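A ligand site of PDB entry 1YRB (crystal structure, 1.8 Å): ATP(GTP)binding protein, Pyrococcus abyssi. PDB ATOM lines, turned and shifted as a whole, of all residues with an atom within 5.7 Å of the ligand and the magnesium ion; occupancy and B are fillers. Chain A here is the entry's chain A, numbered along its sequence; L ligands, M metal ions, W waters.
N of Thr 28 is in hydrogen-bond range of O5 of the ligand.
An oxygen (O5) of the ligand lies within hydrogen-bond range of the backbone NH of Thr 29 (2.8 Å).
An oxygen (O5) of the ligand is in hydrogen-bond range of the side-chain hydroxyl of Thr 29 (2.6 Å).
The side-chain carboxylate (OD1) of Asp 182 lies within hydrogen-bond range of a nitrogen (N3) of the ligand, at 2.8 Å.
N of Ala 238 is in hydrogen-bond range of O11 of the ligand (2.9 Å).
N of Lys 27 sits at hydrogen-bond distance from O3 of the ligand, 2.9 Å away.
The side-chain amino group (NZ) of Lys 27 is in salt-bridge range of an oxygen (O3) of the ligand (2.9 Å).
The backbone NH of Gly 24 sits at hydrogen-bond distance from an oxygen (O2) of the ligand (2.9 Å).
An oxygen (O3) of the ligand sits at hydrogen-bond distance from the backbone NH (N) of Gly 26.
A nitrogen (N2) of the ligand sits close to the side-chain amide oxygen (OD1) of Asn 179 (3.2 Å).
N of Lys 180 lies close to O11 of the ligand.
NZ of Lys 180 is in hydrogen-bond range of O8 of the ligand.
The side-chain hydroxyl (OG) of Ser 237 lies within hydrogen-bond range of an oxygen (O11) of the ligand.
N of Lys 239 is in hydrogen-bond range of O11 of the ligand, at 3.4 Å.
The backbone NH of Ser 25 is in hydrogen-bond range of an oxygen (O3) of the ligand (3.4 Å).
OG1 of Thr 28 sits close to OD2 of Asp 115 (2.8 Å).
The side-chain hydroxyl (OG) of Ser 237 sits at hydrogen-bond distance from the side-chain carboxylate (OD1) of Asp 182 (2.5 Å).
The backbone NH of Ala 238 lies close to the side-chain amide nitrogen of Asn 179 (3.1 Å).
NZ of Lys 27 lies within hydrogen-bond range of O of Gly 118, at 2.9 Å.
NZ of Lys 27 is in hydrogen-bond range of O of Gly 21.
The backbone carbonyl oxygen of Leu 236 lies close to the side-chain amide nitrogen of Asn 179, at 3.4 Å.
The side-chain hydroxyl (OG) of Ser 237 lies close to the backbone NH (N) of Lys 239 (3.2 Å).
N of Thr 240 sits at hydrogen-bond distance from OG of Ser 237, 3.1 Å away.
Merely in contact with the ligand: Leu 183 (3.5 Å), Thr 22 (3.8 Å) and Ala 23 (3.9 Å).
Hydrophobic or aromatic side chains within 4 Å of the ligand: Leu 183 and Ala 238.
Within 4 Å of the ligand: Thr 22, Ala 23, Gly 24, Ser 25, Gly 26, Lys 27, Thr 28, Thr 29, Asn 179, Lys 180, Asp 182, Leu 183, Ser 237, Ala 238 and Lys 239.
Of the 26 residues printed, 1 comes within 4 Å of the magnesium ion.
The nearest printed residue that does not touch the magnesium ion is Asp 115 (4.2 Å).
Water W3 is bound to the magnesium ion.
An oxygen (O1) of the ligand is bound to the magnesium ion, at 2.0 Å.
Water W5 is bound to the magnesium ion (2.0 Å).
The magnesium ion is bound by OG1 of Thr 28, 2.1 Å away.
The magnesium ion is bound by water W4, at 2.2 Å.
The magnesium ion is bound by water W2 (2.2 Å).
Water W4 bridges OD1 of Asp 115 (2.6 Å) and O of Thr 116 (3.1 Å).
Water W1 lies within hydrogen-bond range of N5 of the ligand (3.0 Å) and NZ of Lys 180 (3.1 Å).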
ATOM      1  N   GLY A  21      -3.311 -17.026 -22.049  1.00  0.00           N
ATOM      2  CA  GLY A  21      -2.679 -15.919 -21.352  1.00  0.00           C
ATOM      3  C   GLY A  21      -3.131 -15.923 -19.913  1.00  0.00           C
ATOM      4  O   GLY A  21      -4.120 -16.565 -19.588  1.00  0.00           O
ATOM      5  N   THR A  22      -2.438 -15.186 -19.044  1.00  0.00           N
ATOM      6  CA  THR A  22      -2.845 -15.188 -17.627  1.00  0.00           C
ATOM      7  C   THR A  22      -4.184 -14.502 -17.441  1.00  0.00           C
ATOM      8  O   THR A  22      -4.631 -13.738 -18.293  1.00  0.00           O
ATOM      9  CB  THR A  22      -1.787 -14.500 -16.720  1.00  0.00           C
ATOM     10  OG1 THR A  22      -2.137 -14.754 -15.347  1.00  0.00           O
ATOM     11  CG2 THR A  22      -1.802 -13.029 -16.942  1.00  0.00           C
ATOM     12  N   ALA A  23      -4.850 -14.770 -16.315  1.00  0.00           N
ATOM     13  CA  ALA A  23      -6.143 -14.126 -16.081  1.00  0.00           C
ATOM     14  C   ALA A  23      -6.048 -12.621 -16.225  1.00  0.00           C
ATOM     15  O   ALA A  23      -5.154 -11.997 -15.659  1.00  0.00           O
ATOM     16  CB  ALA A  23      -6.690 -14.507 -14.697  1.00  0.00           C
ATOM     17  N   GLY A  24      -6.975 -12.032 -16.971  1.00  0.00           N
ATOM     18  CA  GLY A  24      -7.044 -10.582 -17.072  1.00  0.00           C
ATOM     19  C   GLY A  24      -6.270  -9.999 -18.227  1.00  0.00           C
ATOM     20  O   GLY A  24      -6.337  -8.800 -18.455  1.00  0.00           O
ATOM     21  N   SER A  25      -5.546 -10.839 -18.984  1.00  0.00           N
ATOM     22  CA  SER A  25      -4.713 -10.353 -20.092  1.00  0.00           C
ATOM     23  C   SER A  25      -5.488  -9.957 -21.344  1.00  0.00           C
ATOM     24  O   SER A  25      -4.948  -9.233 -22.207  1.00  0.00           O
ATOM     25  CB  SER A  25      -3.607 -11.360 -20.455  1.00  0.00           C
ATOM     26  OG  SER A  25      -4.126 -12.635 -20.778  1.00  0.00           O
ATOM     27  N   GLY A  26      -6.720 -10.460 -21.464  1.00  0.00           N
ATOM     28  CA  GLY A  26      -7.593 -10.097 -22.568  1.00  0.00           C
ATOM     29  C   GLY A  26      -7.989 -11.196 -23.549  1.00  0.00           C
ATOM     30  O   GLY A  26      -8.343 -10.892 -24.694  1.00  0.00           O
ATOM     31  N   LYS A  27      -7.945 -12.450 -23.111  1.00  0.00           N
ATOM     32  CA  LYS A  27      -8.316 -13.577 -23.991  1.00  0.00           C
ATOM     33  C   LYS A  27      -9.733 -13.415 -24.510  1.00  0.00           C
ATOM     34  O   LYS A  27      -9.986 -13.536 -25.716  1.00  0.00           O
ATOM     35  CB  LYS A  27      -8.224 -14.912 -23.267  1.00  0.00           C
ATOM     36  CG  LYS A  27      -6.844 -15.270 -22.692  1.00  0.00           C
ATOM     37  CD  LYS A  27      -6.925 -16.600 -21.938  1.00  0.00           C
ATOM     38  CE  LYS A  27      -7.633 -16.502 -20.579  1.00  0.00           C
ATOM     39  NZ  LYS A  27      -6.823 -15.655 -19.614  1.00  0.00           N
ATOM     40  N   THR A  28     -10.662 -13.168 -23.598  1.00  0.00           N
ATOM     41  CA  THR A  28     -12.087 -13.101 -23.967  1.00  0.00           C
ATOM     42  C   THR A  28     -12.390 -11.909 -24.848  1.00  0.00           C
ATOM     43  O   THR A  28     -13.078 -12.029 -25.865  1.00  0.00           O
ATOM     44  CB  THR A  28     -12.952 -13.129 -22.714  1.00  0.00           C
ATOM     45  OG1 THR A  28     -12.704 -14.359 -22.042  1.00  0.00           O
ATOM     46  CG2 THR A  28     -14.445 -13.008 -23.054  1.00  0.00           C
ATOM     47  N   THR A  29     -11.828 -10.756 -24.483  1.00  0.00           N
ATOM     48  CA  THR A  29     -11.984  -9.545 -25.272  1.00  0.00           C
ATOM     49  C   THR A  29     -11.444  -9.708 -26.678  1.00  0.00           C
ATOM     50  O   THR A  29     -12.094  -9.331 -27.663  1.00  0.00           O
ATOM     51  CB  THR A  29     -11.315  -8.334 -24.573  1.00  0.00           C
ATOM     52  OG1 THR A  29     -11.799  -8.269 -23.239  1.00  0.00           O
ATOM     53  CG2 THR A  29     -11.660  -7.025 -25.300  1.00  0.00           C
ATOM     54  N   LEU A  30     -10.274 -10.334 -26.792  1.00  0.00           N
ATOM     55  CA  LEU A  30      -9.643 -10.547 -28.057  1.00  0.00           C
ATOM     56  C   LEU A  30     -10.400 -11.561 -28.913  1.00  0.00           C
ATOM     57  O   LEU A  30     -10.551 -11.378 -30.103  1.00  0.00           O
ATOM     58  CB  LEU A  30      -8.207 -11.033 -27.819  1.00  0.00           C
ATOM     59  CG  LEU A  30      -7.239 -11.183 -28.969  1.00  0.00           C
ATOM     60  CD1 LEU A  30      -7.204  -9.912 -29.817  1.00  0.00           C
ATOM     61  CD2 LEU A  30      -5.887 -11.396 -28.321  1.00  0.00           C
ATOM     62  N   ASP A  50     -13.992 -21.525 -20.726  1.00  0.00           N
ATOM     63  CA  ASP A  50     -13.943 -20.982 -19.361  1.00  0.00           C
ATOM     64  C   ASP A  50     -15.237 -21.169 -18.593  1.00  0.00           C
ATOM     65  O   ASP A  50     -16.289 -20.673 -19.014  1.00  0.00           O
ATOM     66  CB  ASP A  50     -13.615 -19.482 -19.381  1.00  0.00           C
ATOM     67  CG  ASP A  50     -13.451 -18.953 -17.965  1.00  0.00           C
ATOM     68  OD1 ASP A  50     -12.766 -19.623 -17.175  1.00  0.00           O
ATOM     69  OD2 ASP A  50     -13.993 -17.893 -17.648  1.00  0.00           O
ATOM     70  N   VAL A  53     -16.497 -17.212 -16.263  1.00  0.00           N
ATOM     71  CA  VAL A  53     -16.872 -15.885 -16.743  1.00  0.00           C
ATOM     72  C   VAL A  53     -18.402 -15.701 -16.674  1.00  0.00           C
ATOM     73  O   VAL A  53     -19.136 -16.641 -16.947  1.00  0.00           O
ATOM     74  CB  VAL A  53     -16.327 -15.685 -18.179  1.00  0.00           C
ATOM     75  CG1 VAL A  53     -16.889 -16.743 -19.127  1.00  0.00           C
ATOM     76  CG2 VAL A  53     -16.604 -14.267 -18.689  1.00  0.00           C
ATOM     77  N   ASP A 115     -11.415 -19.650 -26.803  1.00  0.00           N
ATOM     78  CA  ASP A 115     -11.138 -18.816 -25.620  1.00  0.00           C
ATOM     79  C   ASP A 115     -10.944 -19.798 -24.455  1.00  0.00           C
ATOM     80  O   ASP A 115     -11.826 -20.594 -24.162  1.00  0.00           O
ATOM     81  CB  ASP A 115     -12.364 -17.914 -25.414  1.00  0.00           C
ATOM     82  CG  ASP A 115     -12.195 -16.906 -24.319  1.00  0.00           C
ATOM     83  OD1 ASP A 115     -11.071 -16.750 -23.802  1.00  0.00           O
ATOM     84  OD2 ASP A 115     -13.218 -16.262 -23.979  1.00  0.00           O
ATOM     85  N   THR A 116      -9.759 -19.783 -23.846  1.00  0.00           N
ATOM     86  CA  THR A 116      -9.385 -20.834 -22.888  1.00  0.00           C
ATOM     87  C   THR A 116      -9.769 -20.432 -21.445  1.00  0.00           C
ATOM     88  O   THR A 116     -10.240 -19.311 -21.215  1.00  0.00           O
ATOM     89  CB  THR A 116      -7.874 -21.098 -23.004  1.00  0.00           C
ATOM     90  OG1 THR A 116      -7.195 -19.861 -22.893  1.00  0.00           O
ATOM     91  CG2 THR A 116      -7.565 -21.673 -24.384  1.00  0.00           C
ATOM     92  N   GLY A 118      -9.931 -19.026 -17.751  1.00  0.00           N
ATOM     93  CA  GLY A 118      -9.441 -17.705 -17.377  1.00  0.00           C
ATOM     94  C   GLY A 118      -8.035 -17.805 -16.800  1.00  0.00           C
ATOM     95  O   GLY A 118      -7.176 -16.960 -17.058  1.00  0.00           O
ATOM     96  N   ILE A 144      -0.868 -14.320 -25.207  1.00  0.00           N
ATOM     97  CA  ILE A 144      -0.848 -12.887 -24.940  1.00  0.00           C
ATOM     98  C   ILE A 144      -0.378 -12.520 -23.572  1.00  0.00           C
ATOM     99  O   ILE A 144      -0.683 -13.208 -22.593  1.00  0.00           O
ATOM    100  CB  ILE A 144      -2.209 -12.228 -25.241  1.00  0.00           C
ATOM    101  CG1 ILE A 144      -3.305 -12.843 -24.370  1.00  0.00           C
ATOM    102  CG2 ILE A 144      -2.510 -12.308 -26.748  1.00  0.00           C
ATOM    103  CD1 ILE A 144      -4.682 -12.086 -24.445  1.00  0.00           C
ATOM    104  N   ASN A 179      -0.949  -7.769 -25.575  1.00  0.00           N
ATOM    105  CA  ASN A 179      -2.288  -7.219 -25.782  1.00  0.00           C
ATOM    106  C   ASN A 179      -2.304  -5.875 -25.051  1.00  0.00           C
ATOM    107  O   ASN A 179      -1.340  -5.519 -24.380  1.00  0.00           O
ATOM    108  CB  ASN A 179      -3.336  -8.173 -25.222  1.00  0.00           C
ATOM    109  CG  ASN A 179      -4.764  -7.744 -25.531  1.00  0.00           C
ATOM    110  OD1 ASN A 179      -5.663  -7.903 -24.705  1.00  0.00           O
ATOM    111  ND2 ASN A 179      -4.972  -7.175 -26.697  1.00  0.00           N
ATOM    112  N   LYS A 180      -3.409  -5.136 -25.171  1.00  0.00           N
ATOM    113  CA  LYS A 180      -3.589  -3.879 -24.442  1.00  0.00           C
ATOM    114  C   LYS A 180      -2.601  -2.797 -24.869  1.00  0.00           C
ATOM    115  O   LYS A 180      -2.305  -1.875 -24.080  1.00  0.00           O
ATOM    116  CB  LYS A 180      -3.514  -4.071 -22.921  1.00  0.00           C
ATOM    117  CG  LYS A 180      -4.416  -5.170 -22.379  1.00  0.00           C
ATOM    118  CD  LYS A 180      -4.570  -5.130 -20.858  1.00  0.00           C
ATOM    119  CE  LYS A 180      -5.432  -6.244 -20.375  1.00  0.00           C
ATOM    120  NZ  LYS A 180      -5.800  -6.111 -18.936  1.00  0.00           N
ATOM    121  N   VAL A 181      -2.098  -2.876 -26.095  1.00  0.00           N
ATOM    122  CA  VAL A 181      -1.079  -1.920 -26.509  1.00  0.00           C
ATOM    123  C   VAL A 181      -1.654  -0.521 -26.750  1.00  0.00           C
ATOM    124  O   VAL A 181      -0.897   0.438 -26.923  1.00  0.00           O
ATOM    125  CB  VAL A 181      -0.279  -2.361 -27.736  1.00  0.00           C
ATOM    126  CG1 VAL A 181       0.381  -3.748 -27.504  1.00  0.00           C
ATOM    127  CG2 VAL A 181      -1.146  -2.363 -28.973  1.00  0.00           C
ATOM    128  N   ASP A 182      -2.990  -0.413 -26.769  1.00  0.00           N
ATOM    129  CA  ASP A 182      -3.646   0.900 -26.856  1.00  0.00           C
ATOM    130  C   ASP A 182      -3.292   1.770 -25.654  1.00  0.00           C
ATOM    131  O   ASP A 182      -3.324   3.013 -25.727  1.00  0.00           O
ATOM    132  CB  ASP A 182      -5.180   0.774 -26.967  1.00  0.00           C
ATOM    133  CG  ASP A 182      -5.756  -0.166 -25.928  1.00  0.00           C
ATOM    134  OD1 ASP A 182      -5.493  -1.388 -26.045  1.00  0.00           O
ATOM    135  OD2 ASP A 182      -6.468   0.298 -25.009  1.00  0.00           O
ATOM    136  N   LEU A 183      -2.945   1.114 -24.545  1.00  0.00           N
ATOM    137  CA  LEU A 183      -2.605   1.797 -23.314  1.00  0.00           C
ATOM    138  C   LEU A 183      -1.172   2.317 -23.296  1.00  0.00           C
ATOM    139  O   LEU A 183      -0.779   2.992 -22.341  1.00  0.00           O
ATOM    140  CB  LEU A 183      -2.793   0.874 -22.123  1.00  0.00           C
ATOM    141  CG  LEU A 183      -4.192   0.296 -21.896  1.00  0.00           C
ATOM    142  CD1 LEU A 183      -4.212  -0.571 -20.655  1.00  0.00           C
ATOM    143  CD2 LEU A 183      -5.207   1.439 -21.791  1.00  0.00           C
ATOM    144  N   LEU A 236      -0.968  -6.335 -30.137  1.00  0.00           N
ATOM    145  CA  LEU A 236      -2.409  -6.340 -30.329  1.00  0.00           C
ATOM    146  C   LEU A 236      -3.144  -5.408 -29.383  1.00  0.00           C
ATOM    147  O   LEU A 236      -2.707  -5.177 -28.245  1.00  0.00           O
ATOM    148  CB  LEU A 236      -2.958  -7.761 -30.102  1.00  0.00           C
ATOM    149  CG  LEU A 236      -2.406  -8.880 -30.977  1.00  0.00           C
ATOM    150  CD1 LEU A 236      -2.907 -10.257 -30.479  1.00  0.00           C
ATOM    151  CD2 LEU A 236      -2.814  -8.648 -32.425  1.00  0.00           C
ATOM    152  N   SER A 237      -4.300  -4.936 -29.841  1.00  0.00           N
ATOM    153  CA  SER A 237      -5.253  -4.361 -28.940  1.00  0.00           C
ATOM    154  C   SER A 237      -6.615  -4.950 -29.222  1.00  0.00           C
ATOM    155  O   SER A 237      -7.159  -4.733 -30.295  1.00  0.00           O
ATOM    156  CB  SER A 237      -5.362  -2.849 -29.138  1.00  0.00           C
ATOM    157  OG  SER A 237      -6.326  -2.363 -28.235  1.00  0.00           O
ATOM    158  N   ALA A 238      -7.179  -5.649 -28.238  1.00  0.00           N
ATOM    159  CA  ALA A 238      -8.526  -6.215 -28.382  1.00  0.00           C
ATOM    160  C   ALA A 238      -9.557  -5.087 -28.419  1.00  0.00           C
ATOM    161  O   ALA A 238     -10.681  -5.277 -28.870  1.00  0.00           O
ATOM    162  CB  ALA A 238      -8.818  -7.180 -27.219  1.00  0.00           C
ATOM    163  N   LYS A 239      -9.154  -3.910 -27.943  1.00  0.00           N
ATOM    164  CA  LYS A 239     -10.047  -2.761 -27.861  1.00  0.00           C
ATOM    165  C   LYS A 239     -10.126  -2.023 -29.197  1.00  0.00           C
ATOM    166  O   LYS A 239     -11.222  -1.731 -29.689  1.00  0.00           O
ATOM    167  CB  LYS A 239      -9.565  -1.824 -26.741  1.00  0.00           C
ATOM    168  CG  LYS A 239     -10.208  -0.434 -26.740  1.00  0.00           C
ATOM    169  CD  LYS A 239      -9.781   0.351 -25.516  1.00  0.00           C
ATOM    170  CE  LYS A 239     -10.650   1.572 -25.287  1.00  0.00           C
ATOM    171  NZ  LYS A 239     -10.254   2.262 -24.025  1.00  0.00           N
ATOM    172  N   THR A 240      -8.971  -1.761 -29.794  1.00  0.00           N
ATOM    173  CA  THR A 240      -8.862  -0.912 -30.970  1.00  0.00           C
ATOM    174  C   THR A 240      -8.602  -1.656 -32.278  1.00  0.00           C
ATOM    175  O   THR A 240      -8.522  -1.040 -33.335  1.00  0.00           O
ATOM    176  CB  THR A 240      -7.731   0.124 -30.797  1.00  0.00           C
ATOM    177  OG1 THR A 240      -6.451  -0.535 -30.921  1.00  0.00           O
ATOM    178  CG2 THR A 240      -7.827   0.793 -29.430  1.00  0.00           C
HETATM  179  P1  LIG L   1      -9.182 -12.713 -19.779  1.00  0.00           P
HETATM  180  O1  LIG L   1     -10.268 -13.457 -20.571  1.00  0.00           O
HETATM  181  O2  LIG L   1      -9.301 -13.103 -18.322  1.00  0.00           O
HETATM  182  O3  LIG L   1      -7.809 -13.018 -20.284  1.00  0.00           O
HETATM  183  O4  LIG L   1      -9.299 -11.111 -19.972  1.00  0.00           O
HETATM  184  P2  LIG L   1     -10.597 -10.255 -20.402  1.00  0.00           P
HETATM  185  O5  LIG L   1     -10.834 -10.311 -21.867  1.00  0.00           O
HETATM  186  O6  LIG L   1     -11.726 -10.618 -19.511  1.00  0.00           O
HETATM  187  O7  LIG L   1     -10.038  -8.760 -20.137  1.00  0.00           O
HETATM  188  C1  LIG L   1      -9.729  -8.391 -18.792  1.00  0.00           C
HETATM  189  C2  LIG L   1      -9.895  -6.884 -18.719  1.00  0.00           C
HETATM  190  O8  LIG L   1      -8.986  -6.272 -19.623  1.00  0.00           O
HETATM  191  C3  LIG L   1     -11.287  -6.440 -19.163  1.00  0.00           C
HETATM  192  O9  LIG L   1     -11.667  -5.274 -18.416  1.00  0.00           O
HETATM  193  C4  LIG L   1     -11.096  -6.018 -20.585  1.00  0.00           C
HETATM  194  O10 LIG L   1     -12.006  -4.976 -20.950  1.00  0.00           O
HETATM  195  C5  LIG L   1      -9.679  -5.474 -20.560  1.00  0.00           C
HETATM  196  N1  LIG L   1      -9.027  -5.564 -21.873  1.00  0.00           N
HETATM  197  C6  LIG L   1      -8.942  -6.670 -22.648  1.00  0.00           C
HETATM  198  N2  LIG L   1      -8.264  -6.381 -23.778  1.00  0.00           N
HETATM  199  C7  LIG L   1      -7.902  -5.077 -23.725  1.00  0.00           C
HETATM  200  C8  LIG L   1      -7.178  -4.121 -24.586  1.00  0.00           C
HETATM  201  O11 LIG L   1      -6.693  -4.451 -25.687  1.00  0.00           O
HETATM  202  N3  LIG L   1      -7.028  -2.845 -24.153  1.00  0.00           N
HETATM  203  C9  LIG L   1      -7.517  -2.445 -22.976  1.00  0.00           C
HETATM  204  N4  LIG L   1      -7.338  -1.147 -22.616  1.00  0.00           N
HETATM  205  N5  LIG L   1      -8.207  -3.244 -22.138  1.00  0.00           N
HETATM  206  C10 LIG L   1      -8.417  -4.559 -22.463  1.00  0.00           C
HETATM  207 MG    MG M   1     -11.794 -14.742 -20.204  1.00  0.00          MG
HETATM  208  O   HOH W   1      -6.999  -3.279 -19.388  1.00  0.00           O
HETATM  209  O   HOH W   2     -12.936 -13.137 -19.315  1.00  0.00           O
HETATM  210  O   HOH W   3     -13.241 -15.894 -19.734  1.00  0.00           O
HETATM  211  O   HOH W   4     -10.782 -16.299 -21.300  1.00  0.00           O
HETATM  212  O   HOH W   5     -10.990 -15.097 -18.367  1.00  0.00           O
HETATM  213  O   HOH W   6      -8.797   0.397 -20.419  1.00  0.00           O
HETATM  214  O   HOH W   7     -14.094  -9.093 -19.179  1.00  0.00           O
HETATM  215  O   HOH W   8     -10.632 -12.165 -16.058  1.00  0.00           O
